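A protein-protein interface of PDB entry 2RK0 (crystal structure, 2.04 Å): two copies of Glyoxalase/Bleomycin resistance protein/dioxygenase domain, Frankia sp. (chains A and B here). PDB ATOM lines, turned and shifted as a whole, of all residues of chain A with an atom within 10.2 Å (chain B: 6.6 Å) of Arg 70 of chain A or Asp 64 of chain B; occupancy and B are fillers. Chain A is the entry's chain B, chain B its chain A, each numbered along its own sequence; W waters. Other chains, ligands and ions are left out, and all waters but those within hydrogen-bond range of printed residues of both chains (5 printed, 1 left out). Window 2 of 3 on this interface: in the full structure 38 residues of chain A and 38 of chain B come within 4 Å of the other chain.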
ATOM      1  N   THR A  12       2.354  -1.259 -28.273  1.00  0.00           N
ATOM      2  CA  THR A  12       2.691  -1.937 -29.513  1.00  0.00           C
ATOM      3  C   THR A  12       3.310  -3.291 -29.169  1.00  0.00           C
ATOM      4  O   THR A  12       4.243  -3.363 -28.365  1.00  0.00           O
ATOM      5  CB  THR A  12       3.685  -1.095 -30.334  1.00  0.00           C
ATOM      6  OG1 THR A  12       3.021   0.085 -30.801  1.00  0.00           O
ATOM      7  CG2 THR A  12       4.222  -1.891 -31.526  1.00  0.00           C
ATOM      8  N   GLY A  62       9.670  -5.963 -37.281  1.00  0.00           N
ATOM      9  CA  GLY A  62      10.809  -6.850 -37.171  1.00  0.00           C
ATOM     10  C   GLY A  62      10.624  -7.798 -36.006  1.00  0.00           C
ATOM     11  O   GLY A  62       9.506  -8.017 -35.543  1.00  0.00           O
ATOM     12  N   ASP A  64      12.456  -7.231 -33.447  1.00  0.00           N
ATOM     13  CA  ASP A  64      12.845  -6.255 -32.439  1.00  0.00           C
ATOM     14  C   ASP A  64      11.992  -6.231 -31.175  1.00  0.00           C
ATOM     15  O   ASP A  64      10.764  -6.227 -31.222  1.00  0.00           O
ATOM     16  CB  ASP A  64      12.869  -4.866 -33.073  1.00  0.00           C
ATOM     17  CG  ASP A  64      13.604  -4.858 -34.390  1.00  0.00           C
ATOM     18  OD1 ASP A  64      14.810  -5.172 -34.399  1.00  0.00           O
ATOM     19  OD2 ASP A  64      12.977  -4.555 -35.426  1.00  0.00           O
ATOM     20  N   LEU A  65      12.678  -6.201 -30.041  1.00  0.00           N
ATOM     21  CA  LEU A  65      12.030  -6.180 -28.742  1.00  0.00           C
ATOM     22  C   LEU A  65      11.985  -4.764 -28.190  1.00  0.00           C
ATOM     23  O   LEU A  65      12.567  -3.842 -28.753  1.00  0.00           O
ATOM     24  CB  LEU A  65      12.796  -7.077 -27.766  1.00  0.00           C
ATOM     25  CG  LEU A  65      12.765  -8.586 -28.023  1.00  0.00           C
ATOM     26  CD1 LEU A  65      13.700  -9.300 -27.061  1.00  0.00           C
ATOM     27  CD2 LEU A  65      11.346  -9.101 -27.853  1.00  0.00           C
ATOM     28  N   PHE A  66      11.281  -4.605 -27.079  1.00  0.00           N
ATOM     29  CA  PHE A  66      11.179  -3.324 -26.395  1.00  0.00           C
ATOM     30  C   PHE A  66      12.593  -2.889 -25.985  1.00  0.00           C
ATOM     31  O   PHE A  66      13.426  -3.726 -25.650  1.00  0.00           O
ATOM     32  CB  PHE A  66      10.312  -3.508 -25.150  1.00  0.00           C
ATOM     33  CG  PHE A  66      10.361  -2.355 -24.189  1.00  0.00           C
ATOM     34  CD1 PHE A  66       9.579  -1.223 -24.395  1.00  0.00           C
ATOM     35  CD2 PHE A  66      11.153  -2.425 -23.049  1.00  0.00           C
ATOM     36  CE1 PHE A  66       9.584  -0.176 -23.470  1.00  0.00           C
ATOM     37  CE2 PHE A  66      11.168  -1.389 -22.122  1.00  0.00           C
ATOM     38  CZ  PHE A  66      10.380  -0.261 -22.331  1.00  0.00           C
ATOM     39  N   ASP A  67      12.862  -1.586 -26.018  1.00  0.00           N
ATOM     40  CA  ASP A  67      14.173  -1.073 -25.622  1.00  0.00           C
ATOM     41  C   ASP A  67      13.985   0.222 -24.850  1.00  0.00           C
ATOM     42  O   ASP A  67      13.642   1.246 -25.440  1.00  0.00           O
ATOM     43  CB  ASP A  67      15.055  -0.783 -26.843  1.00  0.00           C
ATOM     44  CG  ASP A  67      16.477  -0.363 -26.459  1.00  0.00           C
ATOM     45  OD1 ASP A  67      16.683   0.203 -25.361  1.00  0.00           O
ATOM     46  OD2 ASP A  67      17.396  -0.588 -27.269  1.00  0.00           O
ATOM     47  N   GLU A  68      14.226   0.173 -23.542  1.00  0.00           N
ATOM     48  CA  GLU A  68      14.079   1.334 -22.667  1.00  0.00           C
ATOM     49  C   GLU A  68      14.788   2.595 -23.134  1.00  0.00           C
ATOM     50  O   GLU A  68      14.355   3.694 -22.802  1.00  0.00           O
ATOM     51  CB  GLU A  68      14.588   1.020 -21.254  1.00  0.00           C
ATOM     52  CG  GLU A  68      13.889  -0.121 -20.568  1.00  0.00           C
ATOM     53  CD  GLU A  68      14.619  -1.437 -20.725  1.00  0.00           C
ATOM     54  OE1 GLU A  68      14.831  -1.881 -21.876  1.00  0.00           O
ATOM     55  OE2 GLU A  68      14.980  -2.027 -19.683  1.00  0.00           O
ATOM     56  N   THR A  69      15.889   2.453 -23.874  1.00  0.00           N
ATOM     57  CA  THR A  69      16.630   3.627 -24.330  1.00  0.00           C
ATOM     58  C   THR A  69      15.988   4.349 -25.519  1.00  0.00           C
ATOM     59  O   THR A  69      16.408   5.445 -25.896  1.00  0.00           O
ATOM     60  CB  THR A  69      18.118   3.274 -24.659  1.00  0.00           C
ATOM     61  OG1 THR A  69      18.180   2.256 -25.663  1.00  0.00           O
ATOM     62  CG2 THR A  69      18.819   2.764 -23.411  1.00  0.00           C
ATOM     63  N   ARG A  70      14.965   3.745 -26.108  1.00  0.00           N
ATOM     64  CA  ARG A  70      14.283   4.381 -27.232  1.00  0.00           C
ATOM     65  C   ARG A  70      13.199   5.305 -26.676  1.00  0.00           C
ATOM     66  O   ARG A  70      12.437   4.914 -25.794  1.00  0.00           O
ATOM     67  CB  ARG A  70      13.644   3.325 -28.145  1.00  0.00           C
ATOM     68  CG  ARG A  70      12.844   3.905 -29.321  1.00  0.00           C
ATOM     69  CD  ARG A  70      12.239   2.804 -30.214  1.00  0.00           C
ATOM     70  NE  ARG A  70      13.239   2.044 -30.980  1.00  0.00           N
ATOM     71  CZ  ARG A  70      13.720   2.391 -32.177  1.00  0.00           C
ATOM     72  NH1 ARG A  70      13.306   3.501 -32.786  1.00  0.00           N
ATOM     73  NH2 ARG A  70      14.620   1.616 -32.780  1.00  0.00           N
ATOM     74  N   PRO A  71      13.130   6.553 -27.176  1.00  0.00           N
ATOM     75  CA  PRO A  71      12.106   7.470 -26.681  1.00  0.00           C
ATOM     76  C   PRO A  71      10.740   6.789 -26.707  1.00  0.00           C
ATOM     77  O   PRO A  71      10.428   6.013 -27.624  1.00  0.00           O
ATOM     78  CB  PRO A  71      12.196   8.642 -27.649  1.00  0.00           C
ATOM     79  CG  PRO A  71      13.659   8.666 -27.992  1.00  0.00           C
ATOM     80  CD  PRO A  71      13.977   7.204 -28.193  1.00  0.00           C
ATOM     81  N   GLY A  72       9.937   7.077 -25.692  1.00  0.00           N
ATOM     82  CA  GLY A  72       8.623   6.473 -25.587  1.00  0.00           C
ATOM     83  C   GLY A  72       8.465   5.946 -24.178  1.00  0.00           C
ATOM     84  O   GLY A  72       8.715   6.665 -23.210  1.00  0.00           O
ATOM     85  N   LEU A  73       8.067   4.686 -24.054  1.00  0.00           N
ATOM     86  CA  LEU A  73       7.891   4.090 -22.743  1.00  0.00           C
ATOM     87  C   LEU A  73       9.204   3.632 -22.123  1.00  0.00           C
ATOM     88  O   LEU A  73      10.021   2.980 -22.779  1.00  0.00           O
ATOM     89  CB  LEU A  73       6.948   2.884 -22.821  1.00  0.00           C
ATOM     90  CG  LEU A  73       6.592   2.246 -21.472  1.00  0.00           C
ATOM     91  CD1 LEU A  73       5.696   3.196 -20.675  1.00  0.00           C
ATOM     92  CD2 LEU A  73       5.860   0.924 -21.699  1.00  0.00           C
ATOM     93  N   ASP A  74       9.396   3.992 -20.856  1.00  0.00           N
ATOM     94  CA  ASP A  74      10.557   3.571 -20.087  1.00  0.00           C
ATOM     95  C   ASP A  74      10.010   2.332 -19.372  1.00  0.00           C
ATOM     96  O   ASP A  74      10.613   1.262 -19.393  1.00  0.00           O
ATOM     97  CB  ASP A  74      10.955   4.650 -19.087  1.00  0.00           C
ATOM     98  CG  ASP A  74      12.098   4.210 -18.172  1.00  0.00           C
ATOM     99  OD1 ASP A  74      13.205   3.932 -18.673  1.00  0.00           O
ATOM    100  OD2 ASP A  74      11.878   4.148 -16.951  1.00  0.00           O
ATOM    101  N   HIS A  75       8.852   2.496 -18.738  1.00  0.00           N
ATOM    102  CA  HIS A  75       8.149   1.399 -18.079  1.00  0.00           C
ATOM    103  C   HIS A  75       6.781   1.861 -17.598  1.00  0.00           C
ATOM    104  O   HIS A  75       6.580   3.045 -17.321  1.00  0.00           O
ATOM    105  CB  HIS A  75       8.985   0.773 -16.943  1.00  0.00           C
ATOM    106  CG  HIS A  75       9.165   1.646 -15.740  1.00  0.00           C
ATOM    107  ND1 HIS A  75       8.157   1.886 -14.836  1.00  0.00           N
ATOM    108  CD2 HIS A  75      10.265   2.276 -15.259  1.00  0.00           C
ATOM    109  CE1 HIS A  75       8.626   2.625 -13.840  1.00  0.00           C
ATOM    110  NE2 HIS A  75       9.900   2.872 -14.075  1.00  0.00           N
ATOM    111  N   THR B  12      10.731   7.707 -21.567  1.00  0.00           N
ATOM    112  CA  THR B  12      12.128   7.903 -21.910  1.00  0.00           C
ATOM    113  C   THR B  12      12.194   9.125 -22.820  1.00  0.00           C
ATOM    114  O   THR B  12      11.481   9.197 -23.829  1.00  0.00           O
ATOM    115  CB  THR B  12      12.696   6.682 -22.651  1.00  0.00           C
ATOM    116  OG1 THR B  12      12.875   5.603 -21.721  1.00  0.00           O
ATOM    117  CG2 THR B  12      14.035   7.034 -23.309  1.00  0.00           C
ATOM    118  N   VAL B  13      13.030  10.085 -22.447  1.00  0.00           N
ATOM    119  CA  VAL B  13      13.183  11.318 -23.218  1.00  0.00           C
ATOM    120  C   VAL B  13      14.651  11.606 -23.512  1.00  0.00           C
ATOM    121  O   VAL B  13      15.529  11.245 -22.734  1.00  0.00           O
ATOM    122  CB  VAL B  13      12.573  12.521 -22.457  1.00  0.00           C
ATOM    123  CG1 VAL B  13      11.077  12.293 -22.272  1.00  0.00           C
ATOM    124  CG2 VAL B  13      13.260  12.701 -21.107  1.00  0.00           C
ATOM    125  N   ARG B  14      14.908  12.261 -24.639  1.00  0.00           N
ATOM    126  CA  ARG B  14      16.277  12.573 -25.040  1.00  0.00           C
ATOM    127  C   ARG B  14      16.933  13.619 -24.140  1.00  0.00           C
ATOM    128  O   ARG B  14      18.091  13.480 -23.752  1.00  0.00           O
ATOM    129  CB  ARG B  14      16.297  13.057 -26.494  1.00  0.00           C
ATOM    130  CG  ARG B  14      17.691  13.337 -27.038  1.00  0.00           C
ATOM    131  CD  ARG B  14      17.658  13.468 -28.557  1.00  0.00           C
ATOM    132  NE  ARG B  14      18.994  13.432 -29.146  1.00  0.00           N
ATOM    133  CZ  ARG B  14      19.846  14.452 -29.145  1.00  0.00           C
ATOM    134  NH1 ARG B  14      19.504  15.609 -28.584  1.00  0.00           N
ATOM    135  NH2 ARG B  14      21.040  14.315 -29.710  1.00  0.00           N
ATOM    136  N   HIS B  58      18.220   8.588 -20.516  1.00  0.00           N
ATOM    137  CA  HIS B  58      19.231   7.538 -20.446  1.00  0.00           C
ATOM    138  C   HIS B  58      20.573   8.059 -20.968  1.00  0.00           C
ATOM    139  O   HIS B  58      20.641   8.626 -22.057  1.00  0.00           O
ATOM    140  CB  HIS B  58      18.771   6.336 -21.280  1.00  0.00           C
ATOM    141  CG  HIS B  58      17.554   5.652 -20.734  1.00  0.00           C
ATOM    142  ND1 HIS B  58      17.621   4.485 -20.003  1.00  0.00           N
ATOM    143  CD2 HIS B  58      16.245   5.993 -20.779  1.00  0.00           C
ATOM    144  CE1 HIS B  58      16.406   4.138 -19.621  1.00  0.00           C
ATOM    145  NE2 HIS B  58      15.554   5.035 -20.078  1.00  0.00           N
ATOM    146  N   GLY B  61      21.082   6.988 -24.327  1.00  0.00           N
ATOM    147  CA  GLY B  61      19.942   7.103 -25.215  1.00  0.00           C
ATOM    148  C   GLY B  61      20.125   8.271 -26.166  1.00  0.00           C
ATOM    149  O   GLY B  61      21.240   8.750 -26.366  1.00  0.00           O
ATOM    150  N   GLY B  62      19.026   8.724 -26.761  1.00  0.00           N
ATOM    151  CA  GLY B  62      19.095   9.855 -27.667  1.00  0.00           C
ATOM    152  C   GLY B  62      19.558   9.570 -29.084  1.00  0.00           C
ATOM    153  O   GLY B  62      19.749  10.506 -29.861  1.00  0.00           O
ATOM    154  N   THR B  63      19.743   8.296 -29.425  1.00  0.00           N
ATOM    155  CA  THR B  63      20.172   7.939 -30.772  1.00  0.00           C
ATOM    156  C   THR B  63      19.009   7.414 -31.602  1.00  0.00           C
ATOM    157  O   THR B  63      18.989   7.583 -32.823  1.00  0.00           O
ATOM    158  CB  THR B  63      21.301   6.887 -30.754  1.00  0.00           C
ATOM    159  OG1 THR B  63      20.866   5.717 -30.048  1.00  0.00           O
ATOM    160  CG2 THR B  63      22.538   7.466 -30.083  1.00  0.00           C
ATOM    161  N   ASP B  64      18.046   6.774 -30.946  1.00  0.00           N
ATOM    162  CA  ASP B  64      16.864   6.261 -31.642  1.00  0.00           C
ATOM    163  C   ASP B  64      15.732   7.265 -31.453  1.00  0.00           C
ATOM    164  O   ASP B  64      15.781   8.086 -30.541  1.00  0.00           O
ATOM    165  CB  ASP B  64      16.441   4.895 -31.081  1.00  0.00           C
ATOM    166  CG  ASP B  64      17.400   3.781 -31.465  1.00  0.00           C
ATOM    167  OD1 ASP B  64      17.670   3.619 -32.671  1.00  0.00           O
ATOM    168  OD2 ASP B  64      17.879   3.066 -30.564  1.00  0.00           O
ATOM    169  N   LEU B  65      14.723   7.207 -32.319  1.00  0.00           N
ATOM    170  CA  LEU B  65      13.587   8.117 -32.237  1.00  0.00           C
ATOM    171  C   LEU B  65      12.345   7.378 -31.764  1.00  0.00           C
ATOM    172  O   LEU B  65      12.282   6.142 -31.822  1.00  0.00           O
ATOM    173  CB  LEU B  65      13.283   8.712 -33.614  1.00  0.00           C
ATOM    174  CG  LEU B  65      14.370   9.436 -34.409  1.00  0.00           C
ATOM    175  CD1 LEU B  65      13.797   9.904 -35.740  1.00  0.00           C
ATOM    176  CD2 LEU B  65      14.884  10.609 -33.611  1.00  0.00           C
ATOM    177  N   PHE B  66      11.348   8.126 -31.298  1.00  0.00           N
ATOM    178  CA  PHE B  66      10.107   7.478 -30.897  1.00  0.00           C
ATOM    179  C   PHE B  66       9.598   6.825 -32.179  1.00  0.00           C
ATOM    180  O   PHE B  66       9.546   7.462 -33.234  1.00  0.00           O
ATOM    181  CB  PHE B  66       9.063   8.477 -30.410  1.00  0.00           C
ATOM    182  CG  PHE B  66       7.710   7.862 -30.205  1.00  0.00           C
ATOM    183  CD1 PHE B  66       7.479   7.010 -29.133  1.00  0.00           C
ATOM    184  CD2 PHE B  66       6.687   8.087 -31.123  1.00  0.00           C
ATOM    185  CE1 PHE B  66       6.248   6.384 -28.972  1.00  0.00           C
ATOM    186  CE2 PHE B  66       5.450   7.465 -30.975  1.00  0.00           C
ATOM    187  CZ  PHE B  66       5.231   6.610 -29.895  1.00  0.00           C
ATOM    188  N   ASP B  67       9.231   5.554 -32.090  1.00  0.00           N
ATOM    189  CA  ASP B  67       8.744   4.832 -33.249  1.00  0.00           C
ATOM    190  C   ASP B  67       7.642   3.878 -32.807  1.00  0.00           C
ATOM    191  O   ASP B  67       7.931   2.795 -32.300  1.00  0.00           O
ATOM    192  CB  ASP B  67       9.903   4.050 -33.879  1.00  0.00           C
ATOM    193  CG  ASP B  67       9.503   3.325 -35.151  1.00  0.00           C
ATOM    194  OD1 ASP B  67       8.290   3.213 -35.436  1.00  0.00           O
ATOM    195  OD2 ASP B  67      10.414   2.851 -35.860  1.00  0.00           O
ATOM    196  N   ARG B  70       7.629   0.017 -32.968  1.00  0.00           N
ATOM    197  CA  ARG B  70       8.523  -0.741 -32.083  1.00  0.00           C
ATOM    198  C   ARG B  70       7.783  -1.067 -30.785  1.00  0.00           C
ATOM    199  O   ARG B  70       6.999  -0.251 -30.293  1.00  0.00           O
ATOM    200  CB  ARG B  70       9.760   0.095 -31.751  1.00  0.00           C
ATOM    201  CG  ARG B  70      10.570   0.488 -32.966  1.00  0.00           C
ATOM    202  CD  ARG B  70      11.372  -0.687 -33.476  1.00  0.00           C
ATOM    203  NE  ARG B  70      11.793  -0.496 -34.858  1.00  0.00           N
ATOM    204  CZ  ARG B  70      12.868  -1.065 -35.394  1.00  0.00           C
ATOM    205  NH1 ARG B  70      13.640  -1.860 -34.656  1.00  0.00           N
ATOM    206  NH2 ARG B  70      13.160  -0.849 -36.672  1.00  0.00           N
ATOM    207  N   PRO B  71       8.038  -2.249 -30.199  1.00  0.00           N
ATOM    208  CA  PRO B  71       7.351  -2.617 -28.954  1.00  0.00           C
ATOM    209  C   PRO B  71       7.515  -1.553 -27.876  1.00  0.00           C
ATOM    210  O   PRO B  71       8.580  -0.946 -27.728  1.00  0.00           O
ATOM    211  CB  PRO B  71       8.008  -3.944 -28.571  1.00  0.00           C
ATOM    212  CG  PRO B  71       8.422  -4.513 -29.903  1.00  0.00           C
ATOM    213  CD  PRO B  71       8.997  -3.298 -30.591  1.00  0.00           C
ATOM    214  N   ASP B 118       9.679  14.898 -27.723  1.00  0.00           N
ATOM    215  CA  ASP B 118      10.337  13.740 -28.328  1.00  0.00           C
ATOM    216  C   ASP B 118       9.442  13.044 -29.353  1.00  0.00           C
ATOM    217  O   ASP B 118       9.713  11.922 -29.781  1.00  0.00           O
ATOM    218  CB  ASP B 118      10.748  12.754 -27.237  1.00  0.00           C
ATOM    219  CG  ASP B 118      11.978  13.210 -26.490  1.00  0.00           C
ATOM    220  OD1 ASP B 118      13.090  12.901 -26.954  1.00  0.00           O
ATOM    221  OD2 ASP B 118      11.836  13.895 -25.456  1.00  0.00           O
HETATM  222  O   HOH W   1      16.576   8.077 -25.615  1.00  0.00           O
HETATM  223  O   HOH W   2      14.814   5.487 -34.468  1.00  0.00           O
HETATM  224  O   HOH W   3      11.100   0.246 -27.095  1.00  0.00           O
HETATM  225  O   HOH W   4      19.153   3.228 -28.240  1.00  0.00           O
HETATM  226  O   HOH W   5       9.412   4.121 -29.510  1.00  0.00           O
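A ring nitrogen (NE2) of His 58 of chain B is in hydrogen-bond range of the side-chain carboxylate (OD1) of Asp 74 of chain A (3.0 Å). OD1 of Asp 74 of chain A sits close to OG1 of Thr 12 of chain B, 3.5 Å away. The backbone NH (N) of Thr 12 of chain B lies within hydrogen-bond range of the backbone carbonyl oxygen (O) of Gly 72 of chain A (2.8 Å). O of Glu 68 of chain A lies within hydrogen-bond range of OG1 of Thr 12 of chain B (2.6 Å). The guanidinium group of Arg 70 of chain A lies within salt-bridge range of the side-chain carboxylate of Asp 64 of chain B. The guanidinium group (NH1) of Arg 70 of chain B is in salt-bridge range of the side-chain carboxylate (OD2) of Asp 64 of chain A. O of Leu 65 of chain B sits at hydrogen-bond distance from NH1 of Arg 70 of chain A (3.0 Å). NE2 of His 58 of chain B lies within hydrogen-bond range of O of Glu 68 of chain A, 3.3 Å away.
The side-chain hydroxyl (OG1) of Thr 12 of chain B is in hydrogen-bond range of a ring nitrogen (NE2) of His 58 of chain B (3.2 Å). OD1 of Asp 67 of chain A is in hydrogen-bond range of OG1 of Thr 69 of chain A. The guanidinium group (NE) of Arg 70 of chain B is in salt-bridge range of the side-chain carboxylate (OD2) of Asp 67 of chain B, 3.8 Å away.
Thr 12 of chain A touches Arg 70 of chain B. Pro 71 of chain B touches Thr 12 of chain A. Phe 66 of chain A touches Pro 71 of chain B. Thr 69 of chain A touches Thr 12 of chain B (O to CG2, 3.9 Å). CA of Gly 61 of chain B touches O of Thr 69 of chain A (3.96 Å). Thr 12 of chain B touches Arg 70 of chain A (CB to O, 3.6 Å). Arg 70 of chain A touches Asp 67 of chain B (NH1 to CB, 3.6 Å). Arg 70 of chain A touches Arg 70 of chain B (NE to CG, 3.7 Å). Pro 71 of chain A touches Thr 12 of chain B (CA to O, 3.4 Å). Leu 65 of chain B touches Pro 71 of chain A (C to CD, 3.9 Å).
Printed residues of chain B within 4 Å of Leu 65 of chain A: Pro 71 (3.96 Å). No residue of chain A comes within 4 Å of Gly 62 of chain B. No residue of chain A comes within 4 Å of Thr 63 of chain B. Of the printed residues of chain A, Asp 64 of chain B touches Arg 70 and Pro 71. Asp 67 of chain B touches just one residue of chain A: Arg 70. Of chain A, only Thr 12, Asp 64 and Arg 70 come within 4 Å of Arg 70 of chain B. Of the printed residues of chain A, Pro 71 of chain B touches Thr 12 (3.3 Å), Asp 64 (3.2 Å), Leu 65 (3.96 Å) and Phe 66 (3.5 Å). The nearest residue of chain B that does not touch Arg 70 of chain A is Phe 66 of chain B (4.8 Å). The nearest residue of chain A that does not touch Asp 64 of chain B is Asp 67 of chain A (4.9 Å).
Printed residues of chain A that touch a printed residue of chain B: Thr 12, Asp 64, Leu 65, Phe 66, Glu 68, Thr 69, Arg 70, Pro 71, Gly 72 and Asp 74. Along chain B the printed residues that touch a printed residue of chain A span positions 12 to 71.
Asp 64 of chain A touches Arg 70 of chain B, and with the chains exchanged Arg 70 of chain A touches Asp 64 of chain B. Phe 66 of chain A touches Pro 71 of chain B, and with the chains exchanged Pro 71 of chain A touches Phe 66 of chain B. Arg 70 of chain A touches Leu 65 of chain B, but with the chains exchanged Leu 65 of chain A does not touch Arg 70 of chain B (5.7 Å). Arg 70 of chain A touches its own counterpart, Arg 70 of chain B. Positions printed for both chains: 12, 62, 64, 65, 66, 67, 70 and 71.
Water W1 bridges O of Thr 69 of chain A (2.7 Å) and N of Gly 62 of chain B (2.8 Å). Water W4 bridges OD2 of Asp 64 of chain B and OG1 of Thr 69 of chain A. Water W2 lies within hydrogen-bond range of N of Leu 65 of chain B (2.8 Å) and NH1 of Arg 70 of chain A (3.0 Å). Water W3 bridges the backbone NH (N) of Asp 67 of chain A and the backbone carbonyl oxygen (O) of Pro 71 of chain B. Water W5 bridges O of Pro 71 of chain A and N of Asp 67 of chain B.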
